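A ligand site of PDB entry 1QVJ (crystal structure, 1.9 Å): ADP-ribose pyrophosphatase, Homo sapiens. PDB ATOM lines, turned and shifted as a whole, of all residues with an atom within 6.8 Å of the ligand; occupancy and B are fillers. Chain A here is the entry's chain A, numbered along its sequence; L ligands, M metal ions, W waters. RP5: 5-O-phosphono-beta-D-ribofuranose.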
ATOM      1  N   HIS A 111      24.794  13.806   5.843  1.00  0.00           N
ATOM      2  CA  HIS A 111      24.151  14.560   6.906  1.00  0.00           C
ATOM      3  C   HIS A 111      24.499  16.030   7.086  1.00  0.00           C
ATOM      4  O   HIS A 111      25.663  16.446   6.997  1.00  0.00           O
ATOM      5  CB  HIS A 111      24.374  13.825   8.219  1.00  0.00           C
ATOM      6  CG  HIS A 111      23.666  12.523   8.311  1.00  0.00           C
ATOM      7  ND1 HIS A 111      22.284  12.438   8.374  1.00  0.00           N
ATOM      8  CD2 HIS A 111      24.123  11.254   8.354  1.00  0.00           C
ATOM      9  CE1 HIS A 111      21.933  11.165   8.462  1.00  0.00           C
ATOM     10  NE2 HIS A 111      23.030  10.427   8.449  1.00  0.00           N
ATOM     11  N   ALA A 112      23.466  16.800   7.372  1.00  0.00           N
ATOM     12  CA  ALA A 112      23.587  18.231   7.615  1.00  0.00           C
ATOM     13  C   ALA A 112      22.801  18.495   8.888  1.00  0.00           C
ATOM     14  O   ALA A 112      22.145  17.594   9.428  1.00  0.00           O
ATOM     15  CB  ALA A 112      22.987  19.020   6.461  1.00  0.00           C
ATOM     16  N   ALA A 113      22.913  19.713   9.397  1.00  0.00           N
ATOM     17  CA  ALA A 113      22.212  20.080  10.616  1.00  0.00           C
ATOM     18  C   ALA A 113      21.757  21.518  10.428  1.00  0.00           C
ATOM     19  O   ALA A 113      22.502  22.346   9.890  1.00  0.00           O
ATOM     20  CB  ALA A 113      23.131  19.936  11.831  1.00  0.00           C
ATOM     21  N   ASP A 114      20.527  21.796  10.848  1.00  0.00           N
ATOM     22  CA  ASP A 114      19.923  23.122  10.694  1.00  0.00           C
ATOM     23  C   ASP A 114      19.486  23.671  12.034  1.00  0.00           C
ATOM     24  O   ASP A 114      18.450  23.279  12.577  1.00  0.00           O
ATOM     25  CB  ASP A 114      18.709  23.031   9.745  1.00  0.00           C
ATOM     26  CG  ASP A 114      19.095  22.826   8.282  1.00  0.00           C
ATOM     27  OD1 ASP A 114      19.832  23.689   7.743  1.00  0.00           O
ATOM     28  OD2 ASP A 114      18.674  21.821   7.668  1.00  0.00           O
ATOM     29  N   ARG A 146      22.343  33.566   1.784  1.00  0.00           N
ATOM     30  CA  ARG A 146      23.431  32.839   1.146  1.00  0.00           C
ATOM     31  C   ARG A 146      24.204  33.657   0.124  1.00  0.00           C
ATOM     32  O   ARG A 146      23.606  34.257  -0.782  1.00  0.00           O
ATOM     33  CB  ARG A 146      22.885  31.568   0.480  1.00  0.00           C
ATOM     34  CG  ARG A 146      22.339  30.531   1.461  1.00  0.00           C
ATOM     35  CD  ARG A 146      21.666  29.379   0.734  1.00  0.00           C
ATOM     36  NE  ARG A 146      22.597  28.580  -0.058  1.00  0.00           N
ATOM     37  CZ  ARG A 146      23.271  27.523   0.402  1.00  0.00           C
ATOM     38  NH1 ARG A 146      23.137  27.135   1.668  1.00  0.00           N
ATOM     39  NH2 ARG A 146      24.071  26.842  -0.405  1.00  0.00           N
ATOM     40  N   ASP A 148      26.253  32.591  -2.256  1.00  0.00           N
ATOM     41  CA  ASP A 148      26.182  32.010  -3.585  1.00  0.00           C
ATOM     42  C   ASP A 148      24.911  32.306  -4.389  1.00  0.00           C
ATOM     43  O   ASP A 148      24.988  32.694  -5.554  1.00  0.00           O
ATOM     44  CB  ASP A 148      26.410  30.489  -3.508  1.00  0.00           C
ATOM     45  CG  ASP A 148      25.460  29.800  -2.545  1.00  0.00           C
ATOM     46  OD1 ASP A 148      25.665  28.601  -2.255  1.00  0.00           O
ATOM     47  OD2 ASP A 148      24.499  30.442  -2.069  1.00  0.00           O
ATOM     48  N   ALA A 153      18.030  31.637   4.403  1.00  0.00           N
ATOM     49  CA  ALA A 153      17.951  30.279   4.887  1.00  0.00           C
ATOM     50  C   ALA A 153      18.372  30.135   6.339  1.00  0.00           C
ATOM     51  O   ALA A 153      18.924  31.056   6.945  1.00  0.00           O
ATOM     52  CB  ALA A 153      18.830  29.386   4.012  1.00  0.00           C
ATOM     53  N   ILE A 154      17.938  29.080   6.926  1.00  0.00           N
ATOM     54  CA  ILE A 154      18.540  28.641   8.218  1.00  0.00           C
ATOM     55  C   ILE A 154      20.092  28.473   8.036  1.00  0.00           C
ATOM     56  O   ILE A 154      20.539  27.911   7.019  1.00  0.00           O
ATOM     57  CB  ILE A 154      17.868  27.358   8.742  1.00  0.00           C
ATOM     58  CG1 ILE A 154      16.346  27.484   8.719  1.00  0.00           C
ATOM     59  CG2 ILE A 154      18.349  27.024  10.141  1.00  0.00           C
ATOM     60  CD1 ILE A 154      15.631  26.435   9.526  1.00  0.00           C
ATOM     61  N   PRO A 155      20.793  28.984   9.057  1.00  0.00           N
ATOM     62  CA  PRO A 155      22.249  28.899   8.993  1.00  0.00           C
ATOM     63  C   PRO A 155      22.771  27.500   9.320  1.00  0.00           C
ATOM     64  O   PRO A 155      23.422  27.295  10.359  1.00  0.00           O
ATOM     65  CB  PRO A 155      22.695  29.944  10.030  1.00  0.00           C
ATOM     66  CG  PRO A 155      21.643  29.785  11.089  1.00  0.00           C
ATOM     67  CD  PRO A 155      20.361  29.726  10.258  1.00  0.00           C
ATOM     68  N   GLY A 156      22.482  26.533   8.450  1.00  0.00           N
ATOM     69  CA  GLY A 156      22.930  25.168   8.698  1.00  0.00           C
ATOM     70  C   GLY A 156      24.136  24.778   7.871  1.00  0.00           C
ATOM     71  O   GLY A 156      24.771  25.630   7.237  1.00  0.00           O
ATOM     72  N   GLY A 157      24.478  23.497   7.888  1.00  0.00           N
ATOM     73  CA  GLY A 157      25.634  23.052   7.139  1.00  0.00           C
ATOM     74  C   GLY A 157      25.912  21.588   7.339  1.00  0.00           C
ATOM     75  O   GLY A 157      25.269  20.895   8.126  1.00  0.00           O
ATOM     76  N   MET A 158      26.888  21.095   6.580  1.00  0.00           N
ATOM     77  CA  MET A 158      27.279  19.689   6.637  1.00  0.00           C
ATOM     78  C   MET A 158      27.928  19.328   7.948  1.00  0.00           C
ATOM     79  O   MET A 158      28.735  20.095   8.468  1.00  0.00           O
ATOM     80  CB  MET A 158      28.213  19.317   5.460  1.00  0.00           C
ATOM     81  CG  MET A 158      27.678  19.670   4.052  1.00  0.00           C
ATOM     82  SD  MET A 158      26.146  18.688   3.563  1.00  0.00           S
ATOM     83  CE  MET A 158      26.594  17.005   4.094  1.00  0.00           C
ATOM     84  N   GLU A 172      27.875  25.802  13.208  1.00  0.00           N
ATOM     85  CA  GLU A 172      27.312  26.506  12.054  1.00  0.00           C
ATOM     86  C   GLU A 172      26.596  27.792  12.436  1.00  0.00           C
ATOM     87  O   GLU A 172      26.706  28.794  11.740  1.00  0.00           O
ATOM     88  CB  GLU A 172      26.318  25.622  11.291  1.00  0.00           C
ATOM     89  CG  GLU A 172      26.941  24.558  10.398  1.00  0.00           C
ATOM     90  CD  GLU A 172      27.983  25.113   9.449  1.00  0.00           C
ATOM     91  OE1 GLU A 172      27.842  26.259   8.967  1.00  0.00           O
ATOM     92  OE2 GLU A 172      28.965  24.381   9.177  1.00  0.00           O
ATOM     93  N   VAL A 211      15.928  14.905   2.610  1.00  0.00           N
ATOM     94  CA  VAL A 211      15.635  16.210   2.094  1.00  0.00           C
ATOM     95  C   VAL A 211      15.643  16.135   0.586  1.00  0.00           C
ATOM     96  O   VAL A 211      16.659  15.741  -0.008  1.00  0.00           O
ATOM     97  CB  VAL A 211      16.654  17.287   2.554  1.00  0.00           C
ATOM     98  CG1 VAL A 211      16.478  18.548   1.718  1.00  0.00           C
ATOM     99  CG2 VAL A 211      16.480  17.615   4.034  1.00  0.00           C
ATOM    100  N   ASP A 212      14.529  16.469  -0.040  1.00  0.00           N
ATOM    101  CA  ASP A 212      14.436  16.506  -1.491  1.00  0.00           C
ATOM    102  C   ASP A 212      15.400  17.619  -1.946  1.00  0.00           C
ATOM    103  O   ASP A 212      15.110  18.793  -1.830  1.00  0.00           O
ATOM    104  CB  ASP A 212      13.017  16.846  -1.959  1.00  0.00           C
ATOM    105  CG  ASP A 212      12.893  16.795  -3.470  1.00  0.00           C
ATOM    106  OD1 ASP A 212      13.796  16.244  -4.142  1.00  0.00           O
ATOM    107  OD2 ASP A 212      11.886  17.322  -3.966  1.00  0.00           O
ATOM    108  N   ASP A 213      16.560  17.213  -2.480  1.00  0.00           N
ATOM    109  CA  ASP A 213      17.625  18.141  -2.859  1.00  0.00           C
ATOM    110  C   ASP A 213      18.152  17.894  -4.281  1.00  0.00           C
ATOM    111  O   ASP A 213      18.296  16.744  -4.703  1.00  0.00           O
ATOM    112  CB  ASP A 213      18.730  17.950  -1.817  1.00  0.00           C
ATOM    113  CG  ASP A 213      19.780  19.030  -1.862  1.00  0.00           C
ATOM    114  OD1 ASP A 213      20.564  19.042  -2.817  1.00  0.00           O
ATOM    115  OD2 ASP A 213      19.820  19.863  -0.925  1.00  0.00           O
ATOM    116  N   ARG A 215      20.977  17.825  -5.338  1.00  0.00           N
ATOM    117  CA  ARG A 215      22.254  17.106  -5.305  1.00  0.00           C
ATOM    118  C   ARG A 215      22.061  15.603  -5.144  1.00  0.00           C
ATOM    119  O   ARG A 215      23.010  14.820  -5.270  1.00  0.00           O
ATOM    120  CB  ARG A 215      23.102  17.618  -4.144  1.00  0.00           C
ATOM    121  CG  ARG A 215      23.690  19.007  -4.368  1.00  0.00           C
ATOM    122  CD  ARG A 215      24.334  19.556  -3.085  1.00  0.00           C
ATOM    123  NE  ARG A 215      23.341  19.730  -2.028  1.00  0.00           N
ATOM    124  CZ  ARG A 215      23.587  20.296  -0.855  1.00  0.00           C
ATOM    125  NH1 ARG A 215      24.800  20.746  -0.571  1.00  0.00           N
ATOM    126  NH2 ARG A 215      22.616  20.433   0.032  1.00  0.00           N
ATOM    127  N   MET A 222      20.904  13.903   0.484  1.00  0.00           N
ATOM    128  CA  MET A 222      21.021  14.783   1.633  1.00  0.00           C
ATOM    129  C   MET A 222      20.033  14.399   2.715  1.00  0.00           C
ATOM    130  O   MET A 222      18.905  13.984   2.423  1.00  0.00           O
ATOM    131  CB  MET A 222      20.720  16.241   1.258  1.00  0.00           C
ATOM    132  CG  MET A 222      21.715  16.912   0.326  1.00  0.00           C
ATOM    133  SD  MET A 222      23.442  17.038   1.199  1.00  0.00           S
ATOM    134  CE  MET A 222      22.900  17.818   2.885  1.00  0.00           C
ATOM    135  N   GLU A 223      20.467  14.521   3.971  1.00  0.00           N
ATOM    136  CA  GLU A 223      19.584  14.333   5.113  1.00  0.00           C
ATOM    137  C   GLU A 223      19.907  15.470   6.077  1.00  0.00           C
ATOM    138  O   GLU A 223      21.040  15.973   6.097  1.00  0.00           O
ATOM    139  CB  GLU A 223      19.776  12.975   5.814  1.00  0.00           C
ATOM    140  CG  GLU A 223      19.143  11.813   5.007  1.00  0.00           C
ATOM    141  CD  GLU A 223      18.980  10.515   5.789  1.00  0.00           C
ATOM    142  OE1 GLU A 223      18.980  10.562   7.038  1.00  0.00           O
ATOM    143  OE2 GLU A 223      18.830   9.447   5.151  1.00  0.00           O
ATOM    144  N   THR A 224      18.918  15.894   6.852  1.00  0.00           N
ATOM    145  CA  THR A 224      19.194  16.953   7.797  1.00  0.00           C
ATOM    146  C   THR A 224      18.536  16.691   9.119  1.00  0.00           C
ATOM    147  O   THR A 224      17.682  15.807   9.264  1.00  0.00           O
ATOM    148  CB  THR A 224      18.722  18.355   7.275  1.00  0.00           C
ATOM    149  OG1 THR A 224      19.420  19.388   7.994  1.00  0.00           O
ATOM    150  CG2 THR A 224      17.236  18.551   7.499  1.00  0.00           C
ATOM    151  N   TYR A 263      15.348  29.114   1.338  1.00  0.00           N
ATOM    152  CA  TYR A 263      16.171  28.133   0.641  1.00  0.00           C
ATOM    153  C   TYR A 263      15.735  26.706   0.968  1.00  0.00           C
ATOM    154  O   TYR A 263      15.261  26.407   2.061  1.00  0.00           O
ATOM    155  CB  TYR A 263      17.614  28.305   1.097  1.00  0.00           C
ATOM    156  CG  TYR A 263      18.593  27.178   0.885  1.00  0.00           C
ATOM    157  CD1 TYR A 263      18.981  26.794  -0.405  1.00  0.00           C
ATOM    158  CD2 TYR A 263      19.172  26.532   1.952  1.00  0.00           C
ATOM    159  CE1 TYR A 263      19.923  25.797  -0.614  1.00  0.00           C
ATOM    160  CE2 TYR A 263      20.135  25.541   1.764  1.00  0.00           C
ATOM    161  CZ  TYR A 263      20.505  25.187   0.483  1.00  0.00           C
ATOM    162  OH  TYR A 263      21.468  24.196   0.296  1.00  0.00           O
ATOM    163  N   ALA A 264      15.920  25.824  -0.007  1.00  0.00           N
ATOM    164  CA  ALA A 264      15.605  24.404   0.139  1.00  0.00           C
ATOM    165  C   ALA A 264      14.226  24.134   0.734  1.00  0.00           C
ATOM    166  O   ALA A 264      13.202  24.582   0.204  1.00  0.00           O
ATOM    167  CB  ALA A 264      16.660  23.708   0.974  1.00  0.00           C
ATOM    168  N   SER A 265      14.183  23.385   1.828  1.00  0.00           N
ATOM    169  CA  SER A 265      12.913  23.054   2.459  1.00  0.00           C
ATOM    170  C   SER A 265      12.801  23.757   3.810  1.00  0.00           C
ATOM    171  O   SER A 265      12.020  23.359   4.674  1.00  0.00           O
ATOM    172  CB  SER A 265      12.794  21.535   2.666  1.00  0.00           C
ATOM    173  OG  SER A 265      12.882  20.861   1.419  1.00  0.00           O
ATOM    174  N   HIS A 266      13.574  24.816   3.974  1.00  0.00           N
ATOM    175  CA  HIS A 266      13.547  25.520   5.239  1.00  0.00           C
ATOM    176  C   HIS A 266      12.188  26.104   5.639  1.00  0.00           C
ATOM    177  O   HIS A 266      11.875  26.134   6.817  1.00  0.00           O
ATOM    178  CB  HIS A 266      14.656  26.586   5.239  1.00  0.00           C
ATOM    179  CG  HIS A 266      16.045  26.001   5.197  1.00  0.00           C
ATOM    180  ND1 HIS A 266      17.181  26.758   5.336  1.00  0.00           N
ATOM    181  CD2 HIS A 266      16.455  24.717   5.061  1.00  0.00           C
ATOM    182  CE1 HIS A 266      18.242  25.961   5.302  1.00  0.00           C
ATOM    183  NE2 HIS A 266      17.829  24.717   5.129  1.00  0.00           N
ATOM    184  N   PHE A 269      10.214  23.646   7.629  1.00  0.00           N
ATOM    185  CA  PHE A 269      10.735  23.536   8.974  1.00  0.00           C
ATOM    186  C   PHE A 269      10.212  24.710   9.810  1.00  0.00           C
ATOM    187  O   PHE A 269       9.812  24.547  10.966  1.00  0.00           O
ATOM    188  CB  PHE A 269      12.258  23.574   8.941  1.00  0.00           C
ATOM    189  CG  PHE A 269      12.892  22.473   8.119  1.00  0.00           C
ATOM    190  CD1 PHE A 269      14.232  22.560   7.768  1.00  0.00           C
ATOM    191  CD2 PHE A 269      12.150  21.354   7.710  1.00  0.00           C
ATOM    192  CE1 PHE A 269      14.853  21.552   7.021  1.00  0.00           C
ATOM    193  CE2 PHE A 269      12.756  20.339   6.966  1.00  0.00           C
ATOM    194  CZ  PHE A 269      14.104  20.437   6.618  1.00  0.00           C
HETATM  195  C1  RP5 L   1      19.611  21.282   2.932  1.00  0.00           C
HETATM  196  O4  RP5 L   1      20.965  21.707   2.624  1.00  0.00           O
HETATM  197  C2  RP5 L   1      19.489  21.196   4.481  1.00  0.00           C
HETATM  198  O2  RP5 L   1      18.336  21.864   4.983  1.00  0.00           O
HETATM  199  C3  RP5 L   1      20.815  21.757   5.010  1.00  0.00           C
HETATM  200  O3  RP5 L   1      20.643  23.231   5.349  1.00  0.00           O
HETATM  201  C4  RP5 L   1      21.734  21.777   4.006  1.00  0.00           C
HETATM  202  C5  RP5 L   1      23.282  21.809   3.920  1.00  0.00           C
HETATM  203  O5  RP5 L   1      23.933  21.795   2.574  1.00  0.00           O
HETATM  204  P'  RP5 L   1      24.658  23.295   2.285  1.00  0.00           P
HETATM  205  O1X RP5 L   1      25.633  23.168   1.176  1.00  0.00           O
HETATM  206  O2X RP5 L   1      23.669  24.328   1.958  1.00  0.00           O
HETATM  207  O3X RP5 L   1      25.416  23.688   3.639  1.00  0.00           O
HETATM  208  O1  RP5 L   1      19.351  20.060   2.301  1.00  0.00           O
HETATM  209 MG    MG M   1      26.108  26.128   4.719  1.00  0.00          MG
HETATM  210 MG    MG M   2      29.061  25.025   6.278  1.00  0.00          MG
HETATM  211  O   HOH W   1      16.179  21.626   3.376  1.00  0.00           O
HETATM  212  O   HOH W   2      22.633  25.314   4.743  1.00  0.00           O
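A ring nitrogen (NE2) of His 266 lies within hydrogen-bond range of an oxygen (O2) of the ligand (2.9 Å). The side-chain carboxylate (OD1) of Asp 114 sits at hydrogen-bond distance from an oxygen (O3) of the ligand. The side-chain hydroxyl of Tyr 263 lies within hydrogen-bond range of an oxygen (O2X) of the ligand (2.8 Å). NH1 of Arg 146 lies within salt-bridge range of O2X of the ligand (2.9 Å). The side-chain carboxylate of Asp 213 sits at hydrogen-bond distance from an oxygen (O1) of the ligand, at 3.3 Å. The guanidinium group (NH1) of Arg 215 lies within salt-bridge range of an oxygen (O1X) of the ligand, at 3.1 Å.
OD2 of Asp 114 lies within hydrogen-bond range of OG1 of Thr 224. The backbone NH (N) of Ala 112 lies within hydrogen-bond range of the backbone carbonyl oxygen (O) of Glu 223, 2.9 Å away. The guanidinium group of Arg 215 sits close to the side-chain sulfur of Met 222 (3.7 Å). The guanidinium group (NH2) of Arg 146 is in salt-bridge range of the side-chain carboxylate (OD1) of Asp 148 (3.0 Å). The backbone NH (N) of Val 211 sits at hydrogen-bond distance from the backbone carbonyl oxygen (O) of Met 222, 3.1 Å away. N of Ala 113 sits at hydrogen-bond distance from O of Gly 157, at 2.9 Å. A ring nitrogen (ND1) of His 266 sits at hydrogen-bond distance from the backbone NH (N) of Ile 154, 2.9 Å away. The side-chain carboxylate (OD1) of Asp 114 is in hydrogen-bond range of a ring nitrogen (NE2) of His 266, at 3.4 Å.
Ala 112 touches the ligand. Gly 157 touches the ligand (CA to O3X, 3.6 Å). Met 158 touches the ligand (SD to O5, 3.9 Å). Val 211 touches the ligand. OG1 of Thr 224 touches C2 of the ligand, at 3.95 Å. Within 4 Å of the ligand: Ala 112, Asp 114, Arg 146, Gly 157, Met 158, Val 211, Asp 213, Arg 215, Thr 224, Tyr 263 and His 266. The nearest printed residue that does not touch the ligand is Phe 269 (4.05 Å).
Water W1 bridges an oxygen (O2) of the ligand (2.7 Å) and the backbone NH of Ser 265 (3.1 Å). Water W2 lies within hydrogen-bond range of an oxygen (O3) of the ligand (2.9 Å) and the backbone carbonyl oxygen (O) of Gly 156 (3.3 Å).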
